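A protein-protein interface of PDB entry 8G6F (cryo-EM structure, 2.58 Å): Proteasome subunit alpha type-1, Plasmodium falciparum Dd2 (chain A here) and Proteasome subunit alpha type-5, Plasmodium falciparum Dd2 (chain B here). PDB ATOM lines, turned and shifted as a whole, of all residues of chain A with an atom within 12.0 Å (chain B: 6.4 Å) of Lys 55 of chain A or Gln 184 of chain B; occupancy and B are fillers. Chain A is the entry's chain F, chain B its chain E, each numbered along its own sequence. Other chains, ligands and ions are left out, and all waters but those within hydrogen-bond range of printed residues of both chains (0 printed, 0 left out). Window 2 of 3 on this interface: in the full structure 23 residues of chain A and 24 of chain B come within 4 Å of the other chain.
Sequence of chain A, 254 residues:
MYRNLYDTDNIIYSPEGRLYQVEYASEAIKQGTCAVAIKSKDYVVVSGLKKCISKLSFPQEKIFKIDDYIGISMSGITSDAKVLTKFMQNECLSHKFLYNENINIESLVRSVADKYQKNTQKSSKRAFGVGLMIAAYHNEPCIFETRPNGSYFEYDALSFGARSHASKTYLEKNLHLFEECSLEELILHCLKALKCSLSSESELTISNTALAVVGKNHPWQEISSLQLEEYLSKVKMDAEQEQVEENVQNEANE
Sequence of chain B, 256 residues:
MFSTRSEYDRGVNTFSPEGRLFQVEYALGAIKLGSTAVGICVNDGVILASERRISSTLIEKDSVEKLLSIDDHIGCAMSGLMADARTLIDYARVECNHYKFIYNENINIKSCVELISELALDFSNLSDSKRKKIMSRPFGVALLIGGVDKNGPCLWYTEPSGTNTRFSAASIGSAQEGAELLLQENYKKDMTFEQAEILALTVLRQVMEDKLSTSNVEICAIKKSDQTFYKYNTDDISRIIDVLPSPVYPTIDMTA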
ATOM      1  N   LYS A  50     -30.961   9.324   4.059  1.00  0.00           N
ATOM      2  CA  LYS A  50     -29.654   8.690   4.110  1.00  0.00           C
ATOM      3  C   LYS A  50     -28.725   9.473   5.027  1.00  0.00           C
ATOM      4  O   LYS A  50     -28.702  10.705   5.008  1.00  0.00           O
ATOM      5  CB  LYS A  50     -29.054   8.600   2.709  1.00  0.00           C
ATOM      6  CG  LYS A  50     -29.846   7.725   1.762  1.00  0.00           C
ATOM      7  CD  LYS A  50     -28.995   7.207   0.613  1.00  0.00           C
ATOM      8  CE  LYS A  50     -29.345   7.879  -0.701  1.00  0.00           C
ATOM      9  NZ  LYS A  50     -29.057   6.998  -1.864  1.00  0.00           N
ATOM     10  N   LYS A  51     -27.954   8.747   5.829  1.00  0.00           N
ATOM     11  CA  LYS A  51     -27.105   9.347   6.847  1.00  0.00           C
ATOM     12  C   LYS A  51     -25.740   9.670   6.254  1.00  0.00           C
ATOM     13  O   LYS A  51     -25.040   8.775   5.770  1.00  0.00           O
ATOM     14  CB  LYS A  51     -26.961   8.402   8.038  1.00  0.00           C
ATOM     15  CG  LYS A  51     -26.454   9.067   9.300  1.00  0.00           C
ATOM     16  CD  LYS A  51     -26.273   8.055  10.419  1.00  0.00           C
ATOM     17  CE  LYS A  51     -27.357   8.183  11.481  1.00  0.00           C
ATOM     18  NZ  LYS A  51     -27.714   6.867  12.080  1.00  0.00           N
ATOM     19  N   CYS A  52     -25.363  10.944   6.298  1.00  0.00           N
ATOM     20  CA  CYS A  52     -24.059  11.402   5.840  1.00  0.00           C
ATOM     21  C   CYS A  52     -23.188  11.679   7.058  1.00  0.00           C
ATOM     22  O   CYS A  52     -23.519  12.542   7.878  1.00  0.00           O
ATOM     23  CB  CYS A  52     -24.195  12.657   4.982  1.00  0.00           C
ATOM     24  SG  CYS A  52     -25.732  12.742   4.034  1.00  0.00           S
ATOM     25  N   ILE A  53     -22.077  10.950   7.174  1.00  0.00           N
ATOM     26  CA  ILE A  53     -21.225  11.083   8.352  1.00  0.00           C
ATOM     27  C   ILE A  53     -20.569  12.458   8.385  1.00  0.00           C
ATOM     28  O   ILE A  53     -20.589  13.147   9.410  1.00  0.00           O
ATOM     29  CB  ILE A  53     -20.179   9.954   8.388  1.00  0.00           C
ATOM     30  CG1 ILE A  53     -20.699   8.770   9.201  1.00  0.00           C
ATOM     31  CG2 ILE A  53     -18.874  10.435   9.006  1.00  0.00           C
ATOM     32  CD1 ILE A  53     -22.019   8.217   8.714  1.00  0.00           C
ATOM     33  N   SER A  54     -19.981  12.879   7.269  1.00  0.00           N
ATOM     34  CA  SER A  54     -19.238  14.131   7.227  1.00  0.00           C
ATOM     35  C   SER A  54     -19.265  14.671   5.801  1.00  0.00           C
ATOM     36  O   SER A  54     -19.986  14.164   4.938  1.00  0.00           O
ATOM     37  CB  SER A  54     -17.808  13.925   7.737  1.00  0.00           C
ATOM     38  OG  SER A  54     -17.052  13.134   6.838  1.00  0.00           O
ATOM     39  N   LYS A  55     -18.469  15.713   5.561  1.00  0.00           N
ATOM     40  CA  LYS A  55     -18.484  16.382   4.264  1.00  0.00           C
ATOM     41  C   LYS A  55     -17.998  15.462   3.152  1.00  0.00           C
ATOM     42  O   LYS A  55     -18.551  15.470   2.048  1.00  0.00           O
ATOM     43  CB  LYS A  55     -17.625  17.646   4.329  1.00  0.00           C
ATOM     44  CG  LYS A  55     -17.539  18.426   3.025  1.00  0.00           C
ATOM     45  CD  LYS A  55     -16.307  19.318   2.987  1.00  0.00           C
ATOM     46  CE  LYS A  55     -16.135  20.099   4.277  1.00  0.00           C
ATOM     47  NZ  LYS A  55     -15.267  21.291   4.092  1.00  0.00           N
ATOM     48  N   LEU A  56     -16.958  14.678   3.416  1.00  0.00           N
ATOM     49  CA  LEU A  56     -16.326  13.859   2.392  1.00  0.00           C
ATOM     50  C   LEU A  56     -16.943  12.475   2.264  1.00  0.00           C
ATOM     51  O   LEU A  56     -16.558  11.725   1.365  1.00  0.00           O
ATOM     52  CB  LEU A  56     -14.831  13.723   2.688  1.00  0.00           C
ATOM     53  CG  LEU A  56     -14.064  15.038   2.819  1.00  0.00           C
ATOM     54  CD1 LEU A  56     -12.744  14.812   3.523  1.00  0.00           C
ATOM     55  CD2 LEU A  56     -13.839  15.656   1.459  1.00  0.00           C
ATOM     56  N   SER A  57     -17.888  12.123   3.126  1.00  0.00           N
ATOM     57  CA  SER A  57     -18.475  10.795   3.120  1.00  0.00           C
ATOM     58  C   SER A  57     -19.672  10.738   2.183  1.00  0.00           C
ATOM     59  O   SER A  57     -20.424  11.706   2.042  1.00  0.00           O
ATOM     60  CB  SER A  57     -18.907  10.396   4.529  1.00  0.00           C
ATOM     61  OG  SER A  57     -20.119  11.034   4.881  1.00  0.00           O
ATOM     62  N   PHE A  58     -19.835   9.596   1.534  1.00  0.00           N
ATOM     63  CA  PHE A  58     -21.035   9.359   0.747  1.00  0.00           C
ATOM     64  C   PHE A  58     -22.196   9.006   1.678  1.00  0.00           C
ATOM     65  O   PHE A  58     -21.989   8.345   2.698  1.00  0.00           O
ATOM     66  CB  PHE A  58     -20.815   8.222  -0.246  1.00  0.00           C
ATOM     67  CG  PHE A  58     -19.891   8.566  -1.378  1.00  0.00           C
ATOM     68  CD1 PHE A  58     -18.628   9.074  -1.136  1.00  0.00           C
ATOM     69  CD2 PHE A  58     -20.281   8.363  -2.687  1.00  0.00           C
ATOM     70  CE1 PHE A  58     -17.780   9.380  -2.175  1.00  0.00           C
ATOM     71  CE2 PHE A  58     -19.435   8.668  -3.728  1.00  0.00           C
ATOM     72  CZ  PHE A  58     -18.184   9.177  -3.471  1.00  0.00           C
ATOM     73  N   PRO A  59     -23.420   9.429   1.362  1.00  0.00           N
ATOM     74  CA  PRO A  59     -24.561   9.026   2.190  1.00  0.00           C
ATOM     75  C   PRO A  59     -24.764   7.520   2.153  1.00  0.00           C
ATOM     76  O   PRO A  59     -24.519   6.862   1.141  1.00  0.00           O
ATOM     77  CB  PRO A  59     -25.744   9.769   1.559  1.00  0.00           C
ATOM     78  CG  PRO A  59     -25.137  10.857   0.757  1.00  0.00           C
ATOM     79  CD  PRO A  59     -23.826  10.342   0.283  1.00  0.00           C
ATOM     80  N   GLN A  60     -25.222   6.975   3.274  1.00  0.00           N
ATOM     81  CA  GLN A  60     -25.365   5.535   3.405  1.00  0.00           C
ATOM     82  C   GLN A  60     -26.686   5.060   2.818  1.00  0.00           C
ATOM     83  O   GLN A  60     -27.671   5.799   2.765  1.00  0.00           O
ATOM     84  CB  GLN A  60     -25.272   5.122   4.870  1.00  0.00           C
ATOM     85  CG  GLN A  60     -23.850   4.967   5.359  1.00  0.00           C
ATOM     86  CD  GLN A  60     -23.780   4.502   6.791  1.00  0.00           C
ATOM     87  OE1 GLN A  60     -24.754   3.990   7.338  1.00  0.00           O
ATOM     88  NE2 GLN A  60     -22.623   4.681   7.412  1.00  0.00           N
ATOM     89  N   THR A 205     -32.264  16.801  -0.588  1.00  0.00           N
ATOM     90  CA  THR A 205     -31.567  16.854  -1.862  1.00  0.00           C
ATOM     91  C   THR A 205     -31.430  15.445  -2.421  1.00  0.00           C
ATOM     92  O   THR A 205     -31.693  14.453  -1.741  1.00  0.00           O
ATOM     93  CB  THR A 205     -30.187  17.512  -1.716  1.00  0.00           C
ATOM     94  OG1 THR A 205     -29.439  17.333  -2.926  1.00  0.00           O
ATOM     95  CG2 THR A 205     -29.419  16.912  -0.547  1.00  0.00           C
ATOM     96  N   SER A 207     -28.964  13.747  -2.904  1.00  0.00           N
ATOM     97  CA  SER A 207     -27.910  12.943  -2.297  1.00  0.00           C
ATOM     98  C   SER A 207     -28.379  12.261  -1.018  1.00  0.00           C
ATOM     99  O   SER A 207     -28.032  11.101  -0.772  1.00  0.00           O
ATOM    100  CB  SER A 207     -26.689  13.815  -2.014  1.00  0.00           C
ATOM    101  OG  SER A 207     -25.899  13.963  -3.180  1.00  0.00           O
ATOM    102  N   ASN A 208     -29.162  12.954  -0.195  1.00  0.00           N
ATOM    103  CA  ASN A 208     -29.541  12.458   1.119  1.00  0.00           C
ATOM    104  C   ASN A 208     -30.950  11.879   1.161  1.00  0.00           C
ATOM    105  O   ASN A 208     -31.420  11.514   2.240  1.00  0.00           O
ATOM    106  CB  ASN A 208     -29.410  13.574   2.154  1.00  0.00           C
ATOM    107  CG  ASN A 208     -30.455  14.652   1.980  1.00  0.00           C
ATOM    108  OD1 ASN A 208     -31.018  14.815   0.901  1.00  0.00           O
ATOM    109  ND2 ASN A 208     -30.719  15.397   3.046  1.00  0.00           N
ATOM    110  N   SER B 168     -14.555  10.157  -0.112  1.00  0.00           N
ATOM    111  CA  SER B 168     -13.649  10.672  -1.129  1.00  0.00           C
ATOM    112  C   SER B 168     -12.253  10.884  -0.563  1.00  0.00           C
ATOM    113  O   SER B 168     -11.261  10.673  -1.266  1.00  0.00           O
ATOM    114  CB  SER B 168     -14.191  11.975  -1.708  1.00  0.00           C
ATOM    115  OG  SER B 168     -14.775  12.771  -0.697  1.00  0.00           O
ATOM    116  N   ALA B 169     -12.164  11.295   0.698  1.00  0.00           N
ATOM    117  CA  ALA B 169     -10.902  11.403   1.410  1.00  0.00           C
ATOM    118  C   ALA B 169     -11.170  11.123   2.880  1.00  0.00           C
ATOM    119  O   ALA B 169     -12.186  11.564   3.421  1.00  0.00           O
ATOM    120  CB  ALA B 169     -10.267  12.784   1.227  1.00  0.00           C
ATOM    121  N   ALA B 179      -6.139  15.378  10.662  1.00  0.00           N
ATOM    122  CA  ALA B 179      -6.028  14.957   9.272  1.00  0.00           C
ATOM    123  C   ALA B 179      -7.335  15.188   8.530  1.00  0.00           C
ATOM    124  O   ALA B 179      -7.331  15.654   7.387  1.00  0.00           O
ATOM    125  CB  ALA B 179      -5.621  13.489   9.198  1.00  0.00           C
ATOM    126  N   GLU B 180      -8.465  14.870   9.166  1.00  0.00           N
ATOM    127  CA  GLU B 180      -9.761  15.061   8.531  1.00  0.00           C
ATOM    128  C   GLU B 180     -10.044  16.533   8.287  1.00  0.00           C
ATOM    129  O   GLU B 180     -10.599  16.896   7.248  1.00  0.00           O
ATOM    130  CB  GLU B 180     -10.860  14.451   9.395  1.00  0.00           C
ATOM    131  CG  GLU B 180     -11.121  12.985   9.120  1.00  0.00           C
ATOM    132  CD  GLU B 180     -12.445  12.519   9.690  1.00  0.00           C
ATOM    133  OE1 GLU B 180     -13.134  13.341  10.328  1.00  0.00           O
ATOM    134  OE2 GLU B 180     -12.796  11.334   9.498  1.00  0.00           O
ATOM    135  N   LEU B 181      -9.686  17.397   9.235  1.00  0.00           N
ATOM    136  CA  LEU B 181      -9.884  18.826   9.023  1.00  0.00           C
ATOM    137  C   LEU B 181      -9.073  19.316   7.832  1.00  0.00           C
ATOM    138  O   LEU B 181      -9.589  20.026   6.956  1.00  0.00           O
ATOM    139  CB  LEU B 181      -9.509  19.603  10.284  1.00  0.00           C
ATOM    140  CG  LEU B 181     -10.681  20.161  11.091  1.00  0.00           C
ATOM    141  CD1 LEU B 181     -11.421  21.224  10.293  1.00  0.00           C
ATOM    142  CD2 LEU B 181     -11.627  19.046  11.511  1.00  0.00           C
ATOM    143  N   LEU B 182      -7.794  18.934   7.774  1.00  0.00           N
ATOM    144  CA  LEU B 182      -6.963  19.352   6.650  1.00  0.00           C
ATOM    145  C   LEU B 182      -7.520  18.827   5.333  1.00  0.00           C
ATOM    146  O   LEU B 182      -7.582  19.560   4.340  1.00  0.00           O
ATOM    147  CB  LEU B 182      -5.527  18.870   6.850  1.00  0.00           C
ATOM    148  CG  LEU B 182      -4.775  19.471   8.036  1.00  0.00           C
ATOM    149  CD1 LEU B 182      -3.558  18.629   8.375  1.00  0.00           C
ATOM    150  CD2 LEU B 182      -4.366  20.901   7.739  1.00  0.00           C
ATOM    151  N   LEU B 183      -7.927  17.559   5.305  1.00  0.00           N
ATOM    152  CA  LEU B 183      -8.464  16.982   4.079  1.00  0.00           C
ATOM    153  C   LEU B 183      -9.740  17.690   3.654  1.00  0.00           C
ATOM    154  O   LEU B 183      -9.934  17.976   2.469  1.00  0.00           O
ATOM    155  CB  LEU B 183      -8.725  15.492   4.276  1.00  0.00           C
ATOM    156  CG  LEU B 183      -7.478  14.622   4.367  1.00  0.00           C
ATOM    157  CD1 LEU B 183      -7.788  13.339   5.110  1.00  0.00           C
ATOM    158  CD2 LEU B 183      -6.933  14.332   2.982  1.00  0.00           C
ATOM    159  N   GLN B 184     -10.622  17.985   4.606  1.00  0.00           N
ATOM    160  CA  GLN B 184     -11.865  18.662   4.268  1.00  0.00           C
ATOM    161  C   GLN B 184     -11.595  20.041   3.690  1.00  0.00           C
ATOM    162  O   GLN B 184     -12.247  20.453   2.723  1.00  0.00           O
ATOM    163  CB  GLN B 184     -12.756  18.765   5.504  1.00  0.00           C
ATOM    164  CG  GLN B 184     -13.643  17.558   5.708  1.00  0.00           C
ATOM    165  CD  GLN B 184     -13.953  17.294   7.162  1.00  0.00           C
ATOM    166  OE1 GLN B 184     -13.984  18.214   7.978  1.00  0.00           O
ATOM    167  NE2 GLN B 184     -14.191  16.034   7.496  1.00  0.00           N
ATOM    168  N   GLU B 185     -10.637  20.770   4.260  1.00  0.00           N
ATOM    169  CA  GLU B 185     -10.396  22.126   3.786  1.00  0.00           C
ATOM    170  C   GLU B 185      -9.456  22.194   2.587  1.00  0.00           C
ATOM    171  O   GLU B 185      -9.304  23.279   2.015  1.00  0.00           O
ATOM    172  CB  GLU B 185      -9.843  22.990   4.920  1.00  0.00           C
ATOM    173  CG  GLU B 185      -8.473  22.580   5.420  1.00  0.00           C
ATOM    174  CD  GLU B 185      -8.202  23.054   6.836  1.00  0.00           C
ATOM    175  OE1 GLU B 185      -9.081  23.715   7.425  1.00  0.00           O
ATOM    176  OE2 GLU B 185      -7.107  22.769   7.361  1.00  0.00           O
ATOM    177  N   ASN B 186      -8.830  21.084   2.183  1.00  0.00           N
ATOM    178  CA  ASN B 186      -7.891  21.108   1.068  1.00  0.00           C
ATOM    179  C   ASN B 186      -8.241  20.185  -0.092  1.00  0.00           C
ATOM    180  O   ASN B 186      -7.564  20.251  -1.124  1.00  0.00           O
ATOM    181  CB  ASN B 186      -6.481  20.744   1.560  1.00  0.00           C
ATOM    182  CG  ASN B 186      -5.780  21.904   2.236  1.00  0.00           C
ATOM    183  OD1 ASN B 186      -5.459  21.842   3.422  1.00  0.00           O
ATOM    184  ND2 ASN B 186      -5.529  22.966   1.482  1.00  0.00           N
ATOM    185  N   TYR B 187      -9.260  19.340   0.029  1.00  0.00           N
ATOM    186  CA  TYR B 187      -9.561  18.350  -0.998  1.00  0.00           C
ATOM    187  C   TYR B 187     -10.537  18.908  -2.025  1.00  0.00           C
ATOM    188  O   TYR B 187     -11.475  19.632  -1.681  1.00  0.00           O
ATOM    189  CB  TYR B 187     -10.141  17.083  -0.367  1.00  0.00           C
ATOM    190  CG  TYR B 187     -10.625  16.060  -1.372  1.00  0.00           C
ATOM    191  CD1 TYR B 187      -9.745  15.165  -1.960  1.00  0.00           C
ATOM    192  CD2 TYR B 187     -11.961  15.990  -1.732  1.00  0.00           C
ATOM    193  CE1 TYR B 187     -10.182  14.234  -2.875  1.00  0.00           C
ATOM    194  CE2 TYR B 187     -12.404  15.066  -2.648  1.00  0.00           C
ATOM    195  CZ  TYR B 187     -11.511  14.191  -3.215  1.00  0.00           C
ATOM    196  OH  TYR B 187     -11.953  13.264  -4.129  1.00  0.00           O
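The side-chain amino group (NZ) of Lys 55 of chain A lies within hydrogen-bond range of the backbone carbonyl oxygen (O) of Gln 184 of chain B (3.4 Å). OG of Ser 168 of chain B lies within hydrogen-bond range of O of Leu 56 of chain A, 2.9 Å away.
Printed residues of chain B within 4 Å of Lys 55 of chain A: Gln 184 (3.4 Å). Of the printed residues of chain B, Leu 56 of chain A touches Ser 168 (2.9 Å), Ala 169 (3.3 Å), Gln 184 (3.6 Å) and Tyr 187 (3.7 Å). Printed residues of chain B within 4 Å of Phe 58 of chain A: Ser 168. Gln 60 of chain A touches none of the printed residues of chain B. Asn 208 of chain A touches none of the printed residues of chain B. Of the printed residues of chain A, Ser 168 of chain B touches Leu 56 and Phe 58. No residue of chain A comes within 4 Å of Glu 180 of chain B. No residue of chain A comes within 4 Å of Leu 181 of chain B. No residue of chain A comes within 4 Å of Leu 183 of chain B. Of the printed residues of chain A, Gln 184 of chain B touches Lys 55 and Leu 56. Glu 185 of chain B touches none of the printed residues of chain A. No residue of chain A comes within 4 Å of Asn 186 of chain B. Of the printed residues of chain A, Tyr 187 of chain B touches Leu 56. The nearest residue of chain B that does not touch Lys 55 of chain A is Glu 185 of chain B (4.7 Å). The nearest residue of chain A that does not touch Gln 184 of chain B is Ser 54 of chain A (4.1 Å).
Among the printed residues, merely in contact across the chains: Leu 56 of chain A with Ala 169 of chain B (3.3 Å), Leu 56 of chain A with Gln 184 of chain B (3.6 Å), Leu 56 of chain A with Tyr 187 of chain B (3.7 Å) and Phe 58 of chain A with Ser 168 of chain B (3.9 Å).
Of the 11 printed residues of chain B, 4 touch a printed residue of chain A. Hydrophobic or aromatic side chains of chain B within 4 Å of the printed part of chain A: Ala 169 and Tyr 187. Hydrophobic or aromatic side chains of chain A that line the printed part of chain B: Leu 56 and Phe 58. Among the printed residues, 6 pairs touch across the chains. Among the printed residues, no Asp or Glu carboxylate lies within 4 Å of a Lys or Arg side-chain nitrogen of the other chain.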
